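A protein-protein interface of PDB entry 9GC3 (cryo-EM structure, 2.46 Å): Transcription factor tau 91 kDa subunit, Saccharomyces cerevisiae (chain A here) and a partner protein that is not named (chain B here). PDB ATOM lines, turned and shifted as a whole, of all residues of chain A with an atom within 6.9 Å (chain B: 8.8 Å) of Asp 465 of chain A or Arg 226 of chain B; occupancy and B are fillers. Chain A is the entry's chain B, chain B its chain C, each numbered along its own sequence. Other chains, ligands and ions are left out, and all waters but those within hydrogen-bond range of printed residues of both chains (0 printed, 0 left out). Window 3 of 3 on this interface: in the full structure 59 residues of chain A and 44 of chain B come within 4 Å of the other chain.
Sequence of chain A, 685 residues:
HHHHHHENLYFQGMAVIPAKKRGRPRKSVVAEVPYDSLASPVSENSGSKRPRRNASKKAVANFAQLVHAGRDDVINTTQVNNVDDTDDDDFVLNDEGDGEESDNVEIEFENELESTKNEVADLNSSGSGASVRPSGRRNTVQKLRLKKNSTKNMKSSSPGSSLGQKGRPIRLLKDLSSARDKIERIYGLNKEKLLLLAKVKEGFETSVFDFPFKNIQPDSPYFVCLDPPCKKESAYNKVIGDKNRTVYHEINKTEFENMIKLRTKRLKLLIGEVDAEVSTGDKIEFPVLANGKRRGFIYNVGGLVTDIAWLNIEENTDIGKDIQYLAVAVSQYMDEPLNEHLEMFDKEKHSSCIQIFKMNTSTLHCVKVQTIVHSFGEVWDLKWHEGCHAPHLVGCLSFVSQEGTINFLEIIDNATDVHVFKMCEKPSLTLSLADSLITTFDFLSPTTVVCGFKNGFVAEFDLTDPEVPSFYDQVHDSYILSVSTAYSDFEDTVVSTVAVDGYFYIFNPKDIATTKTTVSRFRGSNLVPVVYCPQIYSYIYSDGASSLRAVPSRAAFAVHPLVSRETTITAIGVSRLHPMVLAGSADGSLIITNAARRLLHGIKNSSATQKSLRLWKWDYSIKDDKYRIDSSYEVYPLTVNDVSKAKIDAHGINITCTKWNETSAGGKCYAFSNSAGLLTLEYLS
The side-chain carboxylate of Asp 465 of chain A lies within salt-bridge range of the guanidinium group of Arg 226 of chain B, 2.6 Å away. The backbone carbonyl oxygen of Val 468 of chain A lies within hydrogen-bond range of the guanidinium group of Arg 226 of chain B (2.6 Å). The guanidinium group (NE) of Arg 226 of chain B is in hydrogen-bond range of the side-chain hydroxyl (OG) of Ser 470 of chain A, at 3.4 Å. O of Ser 470 of chain A is in hydrogen-bond range of N of Lys 228 of chain B.
O of Glu 460 of chain A is in hydrogen-bond range of N of Ser 470 of chain A (2.8 Å). The side-chain hydroxyl of Thr 464 of chain A is in hydrogen-bond range of the side-chain carboxylate of Asp 462 of chain A, 2.7 Å away. N of Arg 227 of chain B sits close to OG of Ser 225 of chain B, 3.4 Å away.
Among the printed residues, pairs that only touch across the chains: Asp 462 of chain A with Arg 226 of chain B, Val 468 of chain A with Arg 227 of chain B, Val 468 of chain A with Leu 265 of chain B, Pro 469 of chain A with Pro 244 of chain B, Pro 469 of chain A with Leu 265 of chain B, Ser 470 of chain A with Arg 227 of chain B, Ser 470 of chain A with Pro 244 of chain B, Phe 471 of chain A with Lys 228 of chain B and Phe 471 of chain A with Pro 244 of chain B.
Lys 238 of chain A touches none of the printed residues of chain B. No residue of chain B comes within 4 Å of Thr 464 of chain A. Of chain B, only Arg 226 (2.6 Å) comes within 4 Å of Asp 465 of chain A. No residue of chain B comes within 4 Å of Pro 466 of chain A. Of the printed residues of chain B, Val 468 of chain A touches Arg 226 (2.6 Å), Arg 227 (3.9 Å) and Leu 265 (3.8 Å). Of the printed residues of chain B, Pro 469 of chain A touches Pro 244 and Leu 265. Ser 470 of chain A touches just these residues of chain B: Arg 226, Arg 227, Lys 228 and Pro 244. Of chain A, only Asp 462, Asp 465, Val 468 and Ser 470 come within 4 Å of Arg 226 of chain B. Printed residues of chain A within 4 Å of Lys 228 of chain B: Ser 470 (2.8 Å) and Phe 471 (3.99 Å). Of the printed residues of chain A, Pro 244 of chain B touches Pro 469, Ser 470 and Phe 471. Tyr 246 of chain B touches none of the printed residues of chain A. Printed residues of chain A within 4 Å of Leu 265 of chain B: Val 468 (3.8 Å) and Pro 469 (3.8 Å). The nearest residue of chain B that does not touch Asp 465 of chain A is Arg 227 of chain B (4.03 Å). The nearest residue of chain A that does not touch Arg 226 of chain B is Pro 469 of chain A (4.7 Å).
Hydrophobic or aromatic side chains of chain A that line the printed part of chain B: Val 468, Pro 469 and Phe 471. Of the 16 printed residues of chain B, 5 touch a printed residue of chain A. Among the printed residues, 13 pairs touch across the chains. Among the printed residues, Asp or Glu carboxylates within 4 Å of a Lys or Arg side-chain nitrogen of the other chain: Asp 465 of chain A with Arg 226 of chain B (2.6 Å).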
ATOM      1  N   LYS A 238      28.548 -19.207  -5.801  1.00  0.00           N
ATOM      2  CA  LYS A 238      27.925 -19.745  -7.032  1.00  0.00           C
ATOM      3  C   LYS A 238      27.179 -18.623  -7.751  1.00  0.00           C
ATOM      4  O   LYS A 238      27.370 -18.475  -8.977  1.00  0.00           O
ATOM      5  CB  LYS A 238      26.980 -20.888  -6.686  1.00  0.00           C
ATOM      6  CG  LYS A 238      27.610 -22.081  -5.990  1.00  0.00           C
ATOM      7  CD  LYS A 238      26.706 -23.293  -6.089  1.00  0.00           C
ATOM      8  CE  LYS A 238      27.220 -24.508  -5.347  1.00  0.00           C
ATOM      9  NZ  LYS A 238      26.681 -24.576  -3.967  1.00  0.00           N
ATOM     10  N   LEU A 431      17.226 -10.992 -13.520  1.00  0.00           N
ATOM     11  CA  LEU A 431      16.519 -12.036 -14.286  1.00  0.00           C
ATOM     12  C   LEU A 431      15.431 -11.373 -15.117  1.00  0.00           C
ATOM     13  O   LEU A 431      14.647 -10.609 -14.577  1.00  0.00           O
ATOM     14  CB  LEU A 431      15.886 -13.064 -13.354  1.00  0.00           C
ATOM     15  CG  LEU A 431      16.798 -13.655 -12.281  1.00  0.00           C
ATOM     16  CD1 LEU A 431      15.983 -14.559 -11.382  1.00  0.00           C
ATOM     17  CD2 LEU A 431      18.005 -14.368 -12.865  1.00  0.00           C
ATOM     18  N   THR A 447      19.874 -21.796  -5.632  1.00  0.00           N
ATOM     19  CA  THR A 447      20.368 -21.363  -6.963  1.00  0.00           C
ATOM     20  C   THR A 447      19.269 -21.392  -8.029  1.00  0.00           C
ATOM     21  O   THR A 447      19.613 -21.203  -9.201  1.00  0.00           O
ATOM     22  CB  THR A 447      21.556 -22.233  -7.375  1.00  0.00           C
ATOM     23  OG1 THR A 447      21.156 -23.608  -7.390  1.00  0.00           O
ATOM     24  CG2 THR A 447      22.728 -22.075  -6.432  1.00  0.00           C
ATOM     25  N   THR A 448      18.009 -21.644  -7.667  1.00  0.00           N
ATOM     26  CA  THR A 448      16.918 -21.574  -8.646  1.00  0.00           C
ATOM     27  C   THR A 448      15.721 -20.856  -8.059  1.00  0.00           C
ATOM     28  O   THR A 448      15.412 -21.086  -6.877  1.00  0.00           O
ATOM     29  CB  THR A 448      16.500 -22.939  -9.209  1.00  0.00           C
ATOM     30  OG1 THR A 448      15.748 -23.652  -8.238  1.00  0.00           O
ATOM     31  CG2 THR A 448      17.679 -23.757  -9.683  1.00  0.00           C
ATOM     32  N   GLU A 460      11.191 -21.181 -14.532  1.00  0.00           N
ATOM     33  CA  GLU A 460      12.274 -21.381 -13.556  1.00  0.00           C
ATOM     34  C   GLU A 460      13.545 -20.763 -14.116  1.00  0.00           C
ATOM     35  O   GLU A 460      13.834 -20.977 -15.281  1.00  0.00           O
ATOM     36  CB  GLU A 460      12.446 -22.848 -13.215  1.00  0.00           C
ATOM     37  CG  GLU A 460      13.649 -23.137 -12.346  1.00  0.00           C
ATOM     38  CD  GLU A 460      14.032 -24.610 -12.338  1.00  0.00           C
ATOM     39  OE1 GLU A 460      13.208 -25.435 -11.843  1.00  0.00           O
ATOM     40  OE2 GLU A 460      15.139 -24.935 -12.871  1.00  0.00           O
ATOM     41  N   PHE A 461      14.298 -20.043 -13.290  1.00  0.00           N
ATOM     42  CA  PHE A 461      15.660 -19.584 -13.651  1.00  0.00           C
ATOM     43  C   PHE A 461      16.692 -20.230 -12.742  1.00  0.00           C
ATOM     44  O   PHE A 461      16.470 -20.369 -11.537  1.00  0.00           O
ATOM     45  CB  PHE A 461      15.780 -18.074 -13.556  1.00  0.00           C
ATOM     46  CG  PHE A 461      15.037 -17.327 -14.628  1.00  0.00           C
ATOM     47  CD1 PHE A 461      15.668 -17.004 -15.817  1.00  0.00           C
ATOM     48  CD2 PHE A 461      13.731 -16.920 -14.436  1.00  0.00           C
ATOM     49  CE1 PHE A 461      15.000 -16.308 -16.811  1.00  0.00           C
ATOM     50  CE2 PHE A 461      13.063 -16.214 -15.420  1.00  0.00           C
ATOM     51  CZ  PHE A 461      13.709 -15.900 -16.603  1.00  0.00           C
ATOM     52  N   ASP A 462      17.805 -20.633 -13.338  1.00  0.00           N
ATOM     53  CA  ASP A 462      19.026 -21.019 -12.601  1.00  0.00           C
ATOM     54  C   ASP A 462      19.809 -19.737 -12.340  1.00  0.00           C
ATOM     55  O   ASP A 462      20.230 -19.105 -13.294  1.00  0.00           O
ATOM     56  CB  ASP A 462      19.837 -22.052 -13.376  1.00  0.00           C
ATOM     57  CG  ASP A 462      21.069 -22.552 -12.629  1.00  0.00           C
ATOM     58  OD1 ASP A 462      21.532 -21.867 -11.676  1.00  0.00           O
ATOM     59  OD2 ASP A 462      21.581 -23.626 -13.009  1.00  0.00           O
ATOM     60  N   LEU A 463      20.058 -19.411 -11.080  1.00  0.00           N
ATOM     61  CA  LEU A 463      20.774 -18.164 -10.701  1.00  0.00           C
ATOM     62  C   LEU A 463      22.241 -18.258 -11.091  1.00  0.00           C
ATOM     63  O   LEU A 463      22.887 -17.207 -11.097  1.00  0.00           O
ATOM     64  CB  LEU A 463      20.657 -17.928  -9.200  1.00  0.00           C
ATOM     65  CG  LEU A 463      19.244 -17.812  -8.649  1.00  0.00           C
ATOM     66  CD1 LEU A 463      19.286 -17.448  -7.173  1.00  0.00           C
ATOM     67  CD2 LEU A 463      18.431 -16.802  -9.451  1.00  0.00           C
ATOM     68  N   THR A 464      22.754 -19.439 -11.419  1.00  0.00           N
ATOM     69  CA  THR A 464      24.155 -19.582 -11.892  1.00  0.00           C
ATOM     70  C   THR A 464      24.232 -19.470 -13.418  1.00  0.00           C
ATOM     71  O   THR A 464      25.356 -19.320 -13.923  1.00  0.00           O
ATOM     72  CB  THR A 464      24.750 -20.903 -11.419  1.00  0.00           C
ATOM     73  OG1 THR A 464      24.145 -21.981 -12.141  1.00  0.00           O
ATOM     74  CG2 THR A 464      24.528 -21.107  -9.944  1.00  0.00           C
ATOM     75  N   ASP A 465      23.102 -19.569 -14.127  1.00  0.00           N
ATOM     76  CA  ASP A 465      23.071 -19.419 -15.604  1.00  0.00           C
ATOM     77  C   ASP A 465      21.783 -18.710 -15.995  1.00  0.00           C
ATOM     78  O   ASP A 465      20.884 -19.284 -16.615  1.00  0.00           O
ATOM     79  CB  ASP A 465      23.238 -20.773 -16.289  1.00  0.00           C
ATOM     80  CG  ASP A 465      23.359 -20.656 -17.802  1.00  0.00           C
ATOM     81  OD1 ASP A 465      23.917 -19.636 -18.276  1.00  0.00           O
ATOM     82  OD2 ASP A 465      22.869 -21.565 -18.495  1.00  0.00           O
ATOM     83  N   PRO A 466      21.653 -17.427 -15.608  1.00  0.00           N
ATOM     84  CA  PRO A 466      20.349 -16.764 -15.592  1.00  0.00           C
ATOM     85  C   PRO A 466      19.759 -16.362 -16.951  1.00  0.00           C
ATOM     86  O   PRO A 466      18.593 -16.019 -16.972  1.00  0.00           O
ATOM     87  CB  PRO A 466      20.652 -15.521 -14.757  1.00  0.00           C
ATOM     88  CG  PRO A 466      22.088 -15.206 -15.086  1.00  0.00           C
ATOM     89  CD  PRO A 466      22.744 -16.560 -15.146  1.00  0.00           C
ATOM     90  N   GLU A 467      20.527 -16.438 -18.036  1.00  0.00           N
ATOM     91  CA  GLU A 467      20.100 -15.883 -19.348  1.00  0.00           C
ATOM     92  C   GLU A 467      18.837 -16.590 -19.855  1.00  0.00           C
ATOM     93  O   GLU A 467      17.967 -15.907 -20.401  1.00  0.00           O
ATOM     94  CB  GLU A 467      21.235 -15.996 -20.357  1.00  0.00           C
ATOM     95  CG  GLU A 467      20.908 -15.395 -21.712  1.00  0.00           C
ATOM     96  CD  GLU A 467      21.960 -15.628 -22.789  1.00  0.00           C
ATOM     97  OE1 GLU A 467      23.156 -15.750 -22.435  1.00  0.00           O
ATOM     98  OE2 GLU A 467      21.584 -15.692 -23.986  1.00  0.00           O
ATOM     99  N   VAL A 468      18.727 -17.903 -19.706  1.00  0.00           N
ATOM    100  CA  VAL A 468      17.607 -18.665 -20.329  1.00  0.00           C
ATOM    101  C   VAL A 468      16.940 -19.526 -19.272  1.00  0.00           C
ATOM    102  O   VAL A 468      17.613 -20.226 -18.523  1.00  0.00           O
ATOM    103  CB  VAL A 468      18.127 -19.514 -21.492  1.00  0.00           C
ATOM    104  CG1 VAL A 468      17.010 -20.293 -22.162  1.00  0.00           C
ATOM    105  CG2 VAL A 468      18.889 -18.658 -22.489  1.00  0.00           C
ATOM    106  N   PRO A 469      15.602 -19.492 -19.166  1.00  0.00           N
ATOM    107  CA  PRO A 469      14.914 -20.268 -18.146  1.00  0.00           C
ATOM    108  C   PRO A 469      14.845 -21.762 -18.473  1.00  0.00           C
ATOM    109  O   PRO A 469      14.913 -22.163 -19.630  1.00  0.00           O
ATOM    110  CB  PRO A 469      13.502 -19.668 -18.143  1.00  0.00           C
ATOM    111  CG  PRO A 469      13.319 -19.234 -19.584  1.00  0.00           C
ATOM    112  CD  PRO A 469      14.678 -18.711 -20.004  1.00  0.00           C
ATOM    113  N   SER A 470      14.742 -22.564 -17.420  1.00  0.00           N
ATOM    114  CA  SER A 470      14.684 -24.039 -17.502  1.00  0.00           C
ATOM    115  C   SER A 470      13.377 -24.441 -18.183  1.00  0.00           C
ATOM    116  O   SER A 470      13.396 -25.414 -18.961  1.00  0.00           O
ATOM    117  CB  SER A 470      14.815 -24.657 -16.145  1.00  0.00           C
ATOM    118  OG  SER A 470      16.000 -24.222 -15.495  1.00  0.00           O
ATOM    119  N   PHE A 471      12.284 -23.744 -17.891  1.00  0.00           N
ATOM    120  CA  PHE A 471      11.014 -23.900 -18.629  1.00  0.00           C
ATOM    121  C   PHE A 471      10.299 -22.568 -18.718  1.00  0.00           C
ATOM    122  O   PHE A 471      10.636 -21.648 -18.001  1.00  0.00           O
ATOM    123  CB  PHE A 471      10.173 -24.979 -17.983  1.00  0.00           C
ATOM    124  CG  PHE A 471       9.597 -24.599 -16.656  1.00  0.00           C
ATOM    125  CD1 PHE A 471       8.437 -23.831 -16.564  1.00  0.00           C
ATOM    126  CD2 PHE A 471      10.182 -25.073 -15.499  1.00  0.00           C
ATOM    127  CE1 PHE A 471       7.914 -23.510 -15.322  1.00  0.00           C
ATOM    128  CE2 PHE A 471       9.656 -24.738 -14.257  1.00  0.00           C
ATOM    129  CZ  PHE A 471       8.534 -23.952 -14.173  1.00  0.00           C
ATOM    130  N   SER B 200      12.059 -36.892 -16.172  1.00  0.00           N
ATOM    131  CA  SER B 200      11.817 -35.552 -15.587  1.00  0.00           C
ATOM    132  C   SER B 200      13.144 -34.800 -15.388  1.00  0.00           C
ATOM    133  O   SER B 200      13.089 -33.576 -15.228  1.00  0.00           O
ATOM    134  CB  SER B 200      11.051 -35.658 -14.312  1.00  0.00           C
ATOM    135  OG  SER B 200      11.815 -36.324 -13.319  1.00  0.00           O
ATOM    136  N   ASN B 201      14.284 -35.480 -15.394  1.00  0.00           N
ATOM    137  CA  ASN B 201      15.613 -34.824 -15.384  1.00  0.00           C
ATOM    138  C   ASN B 201      16.076 -34.497 -16.802  1.00  0.00           C
ATOM    139  O   ASN B 201      17.256 -34.106 -16.970  1.00  0.00           O
ATOM    140  CB  ASN B 201      16.631 -35.678 -14.637  1.00  0.00           C
ATOM    141  CG  ASN B 201      17.045 -36.938 -15.351  1.00  0.00           C
ATOM    142  OD1 ASN B 201      16.665 -37.196 -16.483  1.00  0.00           O
ATOM    143  ND2 ASN B 201      17.829 -37.750 -14.685  1.00  0.00           N
ATOM    144  N   ASN B 202      15.221 -34.732 -17.800  1.00  0.00           N
ATOM    145  CA  ASN B 202      15.497 -34.408 -19.221  1.00  0.00           C
ATOM    146  C   ASN B 202      16.641 -35.234 -19.806  1.00  0.00           C
ATOM    147  O   ASN B 202      17.182 -34.846 -20.884  1.00  0.00           O
ATOM    148  CB  ASN B 202      15.817 -32.930 -19.374  1.00  0.00           C
ATOM    149  CG  ASN B 202      14.809 -32.053 -18.666  1.00  0.00           C
ATOM    150  OD1 ASN B 202      13.618 -32.068 -19.000  1.00  0.00           O
ATOM    151  ND2 ASN B 202      15.289 -31.299 -17.689  1.00  0.00           N
ATOM    152  N   SER B 203      16.972 -36.364 -19.194  1.00  0.00           N
ATOM    153  CA  SER B 203      17.739 -37.421 -19.885  1.00  0.00           C
ATOM    154  C   SER B 203      16.784 -38.166 -20.830  1.00  0.00           C
ATOM    155  O   SER B 203      15.598 -38.355 -20.482  1.00  0.00           O
ATOM    156  CB  SER B 203      18.410 -38.325 -18.909  1.00  0.00           C
ATOM    157  OG  SER B 203      17.455 -38.976 -18.083  1.00  0.00           O
ATOM    158  N   GLN B 222      20.683 -38.734 -24.552  1.00  0.00           N
ATOM    159  CA  GLN B 222      20.955 -37.340 -24.127  1.00  0.00           C
ATOM    160  C   GLN B 222      21.102 -37.314 -22.617  1.00  0.00           C
ATOM    161  O   GLN B 222      20.255 -37.904 -21.907  1.00  0.00           O
ATOM    162  CB  GLN B 222      19.844 -36.390 -24.565  1.00  0.00           C
ATOM    163  CG  GLN B 222      20.191 -34.933 -24.304  1.00  0.00           C
ATOM    164  CD  GLN B 222      19.152 -33.981 -24.841  1.00  0.00           C
ATOM    165  OE1 GLN B 222      19.277 -33.474 -25.955  1.00  0.00           O
ATOM    166  NE2 GLN B 222      18.123 -33.741 -24.032  1.00  0.00           N
ATOM    167  N   ASN B 223      22.134 -36.640 -22.127  1.00  0.00           N
ATOM    168  CA  ASN B 223      22.381 -36.545 -20.664  1.00  0.00           C
ATOM    169  C   ASN B 223      21.337 -35.635 -20.022  1.00  0.00           C
ATOM    170  O   ASN B 223      20.738 -34.771 -20.724  1.00  0.00           O
ATOM    171  CB  ASN B 223      23.798 -36.087 -20.351  1.00  0.00           C
ATOM    172  CG  ASN B 223      24.846 -37.032 -20.901  1.00  0.00           C
ATOM    173  OD1 ASN B 223      24.694 -38.248 -20.820  1.00  0.00           O
ATOM    174  ND2 ASN B 223      25.921 -36.488 -21.454  1.00  0.00           N
ATOM    175  N   ALA B 224      21.152 -35.797 -18.718  1.00  0.00           N
ATOM    176  CA  ALA B 224      20.284 -34.936 -17.891  1.00  0.00           C
ATOM    177  C   ALA B 224      20.718 -33.472 -18.004  1.00  0.00           C
ATOM    178  O   ALA B 224      21.930 -33.171 -18.174  1.00  0.00           O
ATOM    179  CB  ALA B 224      20.310 -35.375 -16.459  1.00  0.00           C
ATOM    180  N   SER B 225      19.738 -32.587 -17.920  1.00  0.00           N
ATOM    181  CA  SER B 225      19.908 -31.138 -18.142  1.00  0.00           C
ATOM    182  C   SER B 225      18.771 -30.410 -17.443  1.00  0.00           C
ATOM    183  O   SER B 225      17.717 -31.001 -17.174  1.00  0.00           O
ATOM    184  CB  SER B 225      19.928 -30.819 -19.612  1.00  0.00           C
ATOM    185  OG  SER B 225      20.027 -29.419 -19.837  1.00  0.00           O
ATOM    186  N   ARG B 226      18.990 -29.142 -17.146  1.00  0.00           N
ATOM    187  CA  ARG B 226      17.942 -28.321 -16.512  1.00  0.00           C
ATOM    188  C   ARG B 226      16.865 -27.965 -17.534  1.00  0.00           C
ATOM    189  O   ARG B 226      15.714 -27.793 -17.115  1.00  0.00           O
ATOM    190  CB  ARG B 226      18.573 -27.095 -15.887  1.00  0.00           C
ATOM    191  CG  ARG B 226      18.992 -26.017 -16.871  1.00  0.00           C
ATOM    192  CD  ARG B 226      19.322 -24.738 -16.102  1.00  0.00           C
ATOM    193  NE  ARG B 226      19.031 -23.572 -16.929  1.00  0.00           N
ATOM    194  CZ  ARG B 226      19.919 -22.999 -17.703  1.00  0.00           C
ATOM    195  NH1 ARG B 226      19.570 -21.967 -18.451  1.00  0.00           N
ATOM    196  NH2 ARG B 226      21.171 -23.436 -17.707  1.00  0.00           N
ATOM    197  N   ARG B 227      17.223 -27.854 -18.804  1.00  0.00           N
ATOM    198  CA  ARG B 227      16.298 -27.381 -19.863  1.00  0.00           C
ATOM    199  C   ARG B 227      15.184 -28.400 -20.092  1.00  0.00           C
ATOM    200  O   ARG B 227      15.459 -29.450 -20.661  1.00  0.00           O
ATOM    201  CB  ARG B 227      17.090 -27.109 -21.140  1.00  0.00           C
ATOM    202  CG  ARG B 227      18.046 -25.938 -20.994  1.00  0.00           C
ATOM    203  CD  ARG B 227      18.541 -25.395 -22.314  1.00  0.00           C
ATOM    204  NE  ARG B 227      19.112 -24.054 -22.215  1.00  0.00           N
ATOM    205  CZ  ARG B 227      20.334 -23.741 -21.771  1.00  0.00           C
ATOM    206  NH1 ARG B 227      20.719 -22.475 -21.783  1.00  0.00           N
ATOM    207  NH2 ARG B 227      21.162 -24.664 -21.305  1.00  0.00           N
ATOM    208  N   LYS B 228      13.969 -28.087 -19.680  1.00  0.00           N
ATOM    209  CA  LYS B 228      12.861 -29.048 -19.701  1.00  0.00           C
ATOM    210  C   LYS B 228      12.469 -29.373 -21.150  1.00  0.00           C
ATOM    211  O   LYS B 228      12.321 -28.450 -21.975  1.00  0.00           O
ATOM    212  CB  LYS B 228      11.638 -28.561 -18.934  1.00  0.00           C
ATOM    213  CG  LYS B 228      10.547 -29.616 -18.882  1.00  0.00           C
ATOM    214  CD  LYS B 228       9.631 -29.628 -17.713  1.00  0.00           C
ATOM    215  CE  LYS B 228       8.617 -30.743 -17.860  1.00  0.00           C
ATOM    216  NZ  LYS B 228       9.245 -32.084 -17.962  1.00  0.00           N
ATOM    217  N   ILE B 229      12.291 -30.657 -21.444  1.00  0.00           N
ATOM    218  CA  ILE B 229      11.886 -31.121 -22.792  1.00  0.00           C
ATOM    219  C   ILE B 229      10.436 -30.730 -23.015  1.00  0.00           C
ATOM    220  O   ILE B 229       9.573 -31.071 -22.179  1.00  0.00           O
ATOM    221  CB  ILE B 229      12.132 -32.622 -22.969  1.00  0.00           C
ATOM    222  CG1 ILE B 229      13.637 -32.913 -22.889  1.00  0.00           C
ATOM    223  CG2 ILE B 229      11.537 -33.079 -24.296  1.00  0.00           C
ATOM    224  CD1 ILE B 229      13.934 -34.329 -22.527  1.00  0.00           C
ATOM    225  N   CYS B 243      13.216 -27.707 -26.544  1.00  0.00           N
ATOM    226  CA  CYS B 243      13.310 -27.175 -25.174  1.00  0.00           C
ATOM    227  C   CYS B 243      13.463 -25.674 -25.303  1.00  0.00           C
ATOM    228  O   CYS B 243      13.627 -25.178 -26.423  1.00  0.00           O
ATOM    229  CB  CYS B 243      14.469 -27.839 -24.439  1.00  0.00           C
ATOM    230  SG  CYS B 243      16.065 -27.213 -24.997  1.00  0.00           S
ATOM    231  N   PRO B 244      13.367 -24.899 -24.195  1.00  0.00           N
ATOM    232  CA  PRO B 244      13.442 -23.440 -24.300  1.00  0.00           C
ATOM    233  C   PRO B 244      14.696 -22.969 -25.049  1.00  0.00           C
ATOM    234  O   PRO B 244      15.833 -23.257 -24.645  1.00  0.00           O
ATOM    235  CB  PRO B 244      13.392 -22.966 -22.857  1.00  0.00           C
ATOM    236  CG  PRO B 244      12.629 -24.069 -22.155  1.00  0.00           C
ATOM    237  CD  PRO B 244      13.096 -25.348 -22.820  1.00  0.00           C
ATOM    238  N   TYR B 246      15.913 -24.012 -27.917  1.00  0.00           N
ATOM    239  CA  TYR B 246      16.686 -24.980 -28.740  1.00  0.00           C
ATOM    240  C   TYR B 246      15.776 -26.045 -29.323  1.00  0.00           C
ATOM    241  O   TYR B 246      14.740 -26.400 -28.716  1.00  0.00           O
ATOM    242  CB  TYR B 246      17.774 -25.642 -27.908  1.00  0.00           C
ATOM    243  CG  TYR B 246      18.933 -24.743 -27.600  1.00  0.00           C
ATOM    244  CD1 TYR B 246      18.950 -23.963 -26.457  1.00  0.00           C
ATOM    245  CD2 TYR B 246      20.020 -24.685 -28.453  1.00  0.00           C
ATOM    246  CE1 TYR B 246      20.024 -23.137 -26.175  1.00  0.00           C
ATOM    247  CE2 TYR B 246      21.112 -23.879 -28.175  1.00  0.00           C
ATOM    248  CZ  TYR B 246      21.121 -23.113 -27.021  1.00  0.00           C
ATOM    249  OH  TYR B 246      22.178 -22.291 -26.746  1.00  0.00           O
ATOM    250  N   LEU B 265      11.576 -18.273 -26.957  1.00  0.00           N
ATOM    251  CA  LEU B 265      11.477 -19.157 -25.775  1.00  0.00           C
ATOM    252  C   LEU B 265      10.056 -19.699 -25.611  1.00  0.00           C
ATOM    253  O   LEU B 265       9.864 -20.495 -24.670  1.00  0.00           O
ATOM    254  CB  LEU B 265      11.898 -18.381 -24.526  1.00  0.00           C
ATOM    255  CG  LEU B 265      13.342 -17.892 -24.507  1.00  0.00           C
ATOM    256  CD1 LEU B 265      13.590 -17.059 -23.263  1.00  0.00           C
ATOM    257  CD2 LEU B 265      14.328 -19.060 -24.614  1.00  0.00           C
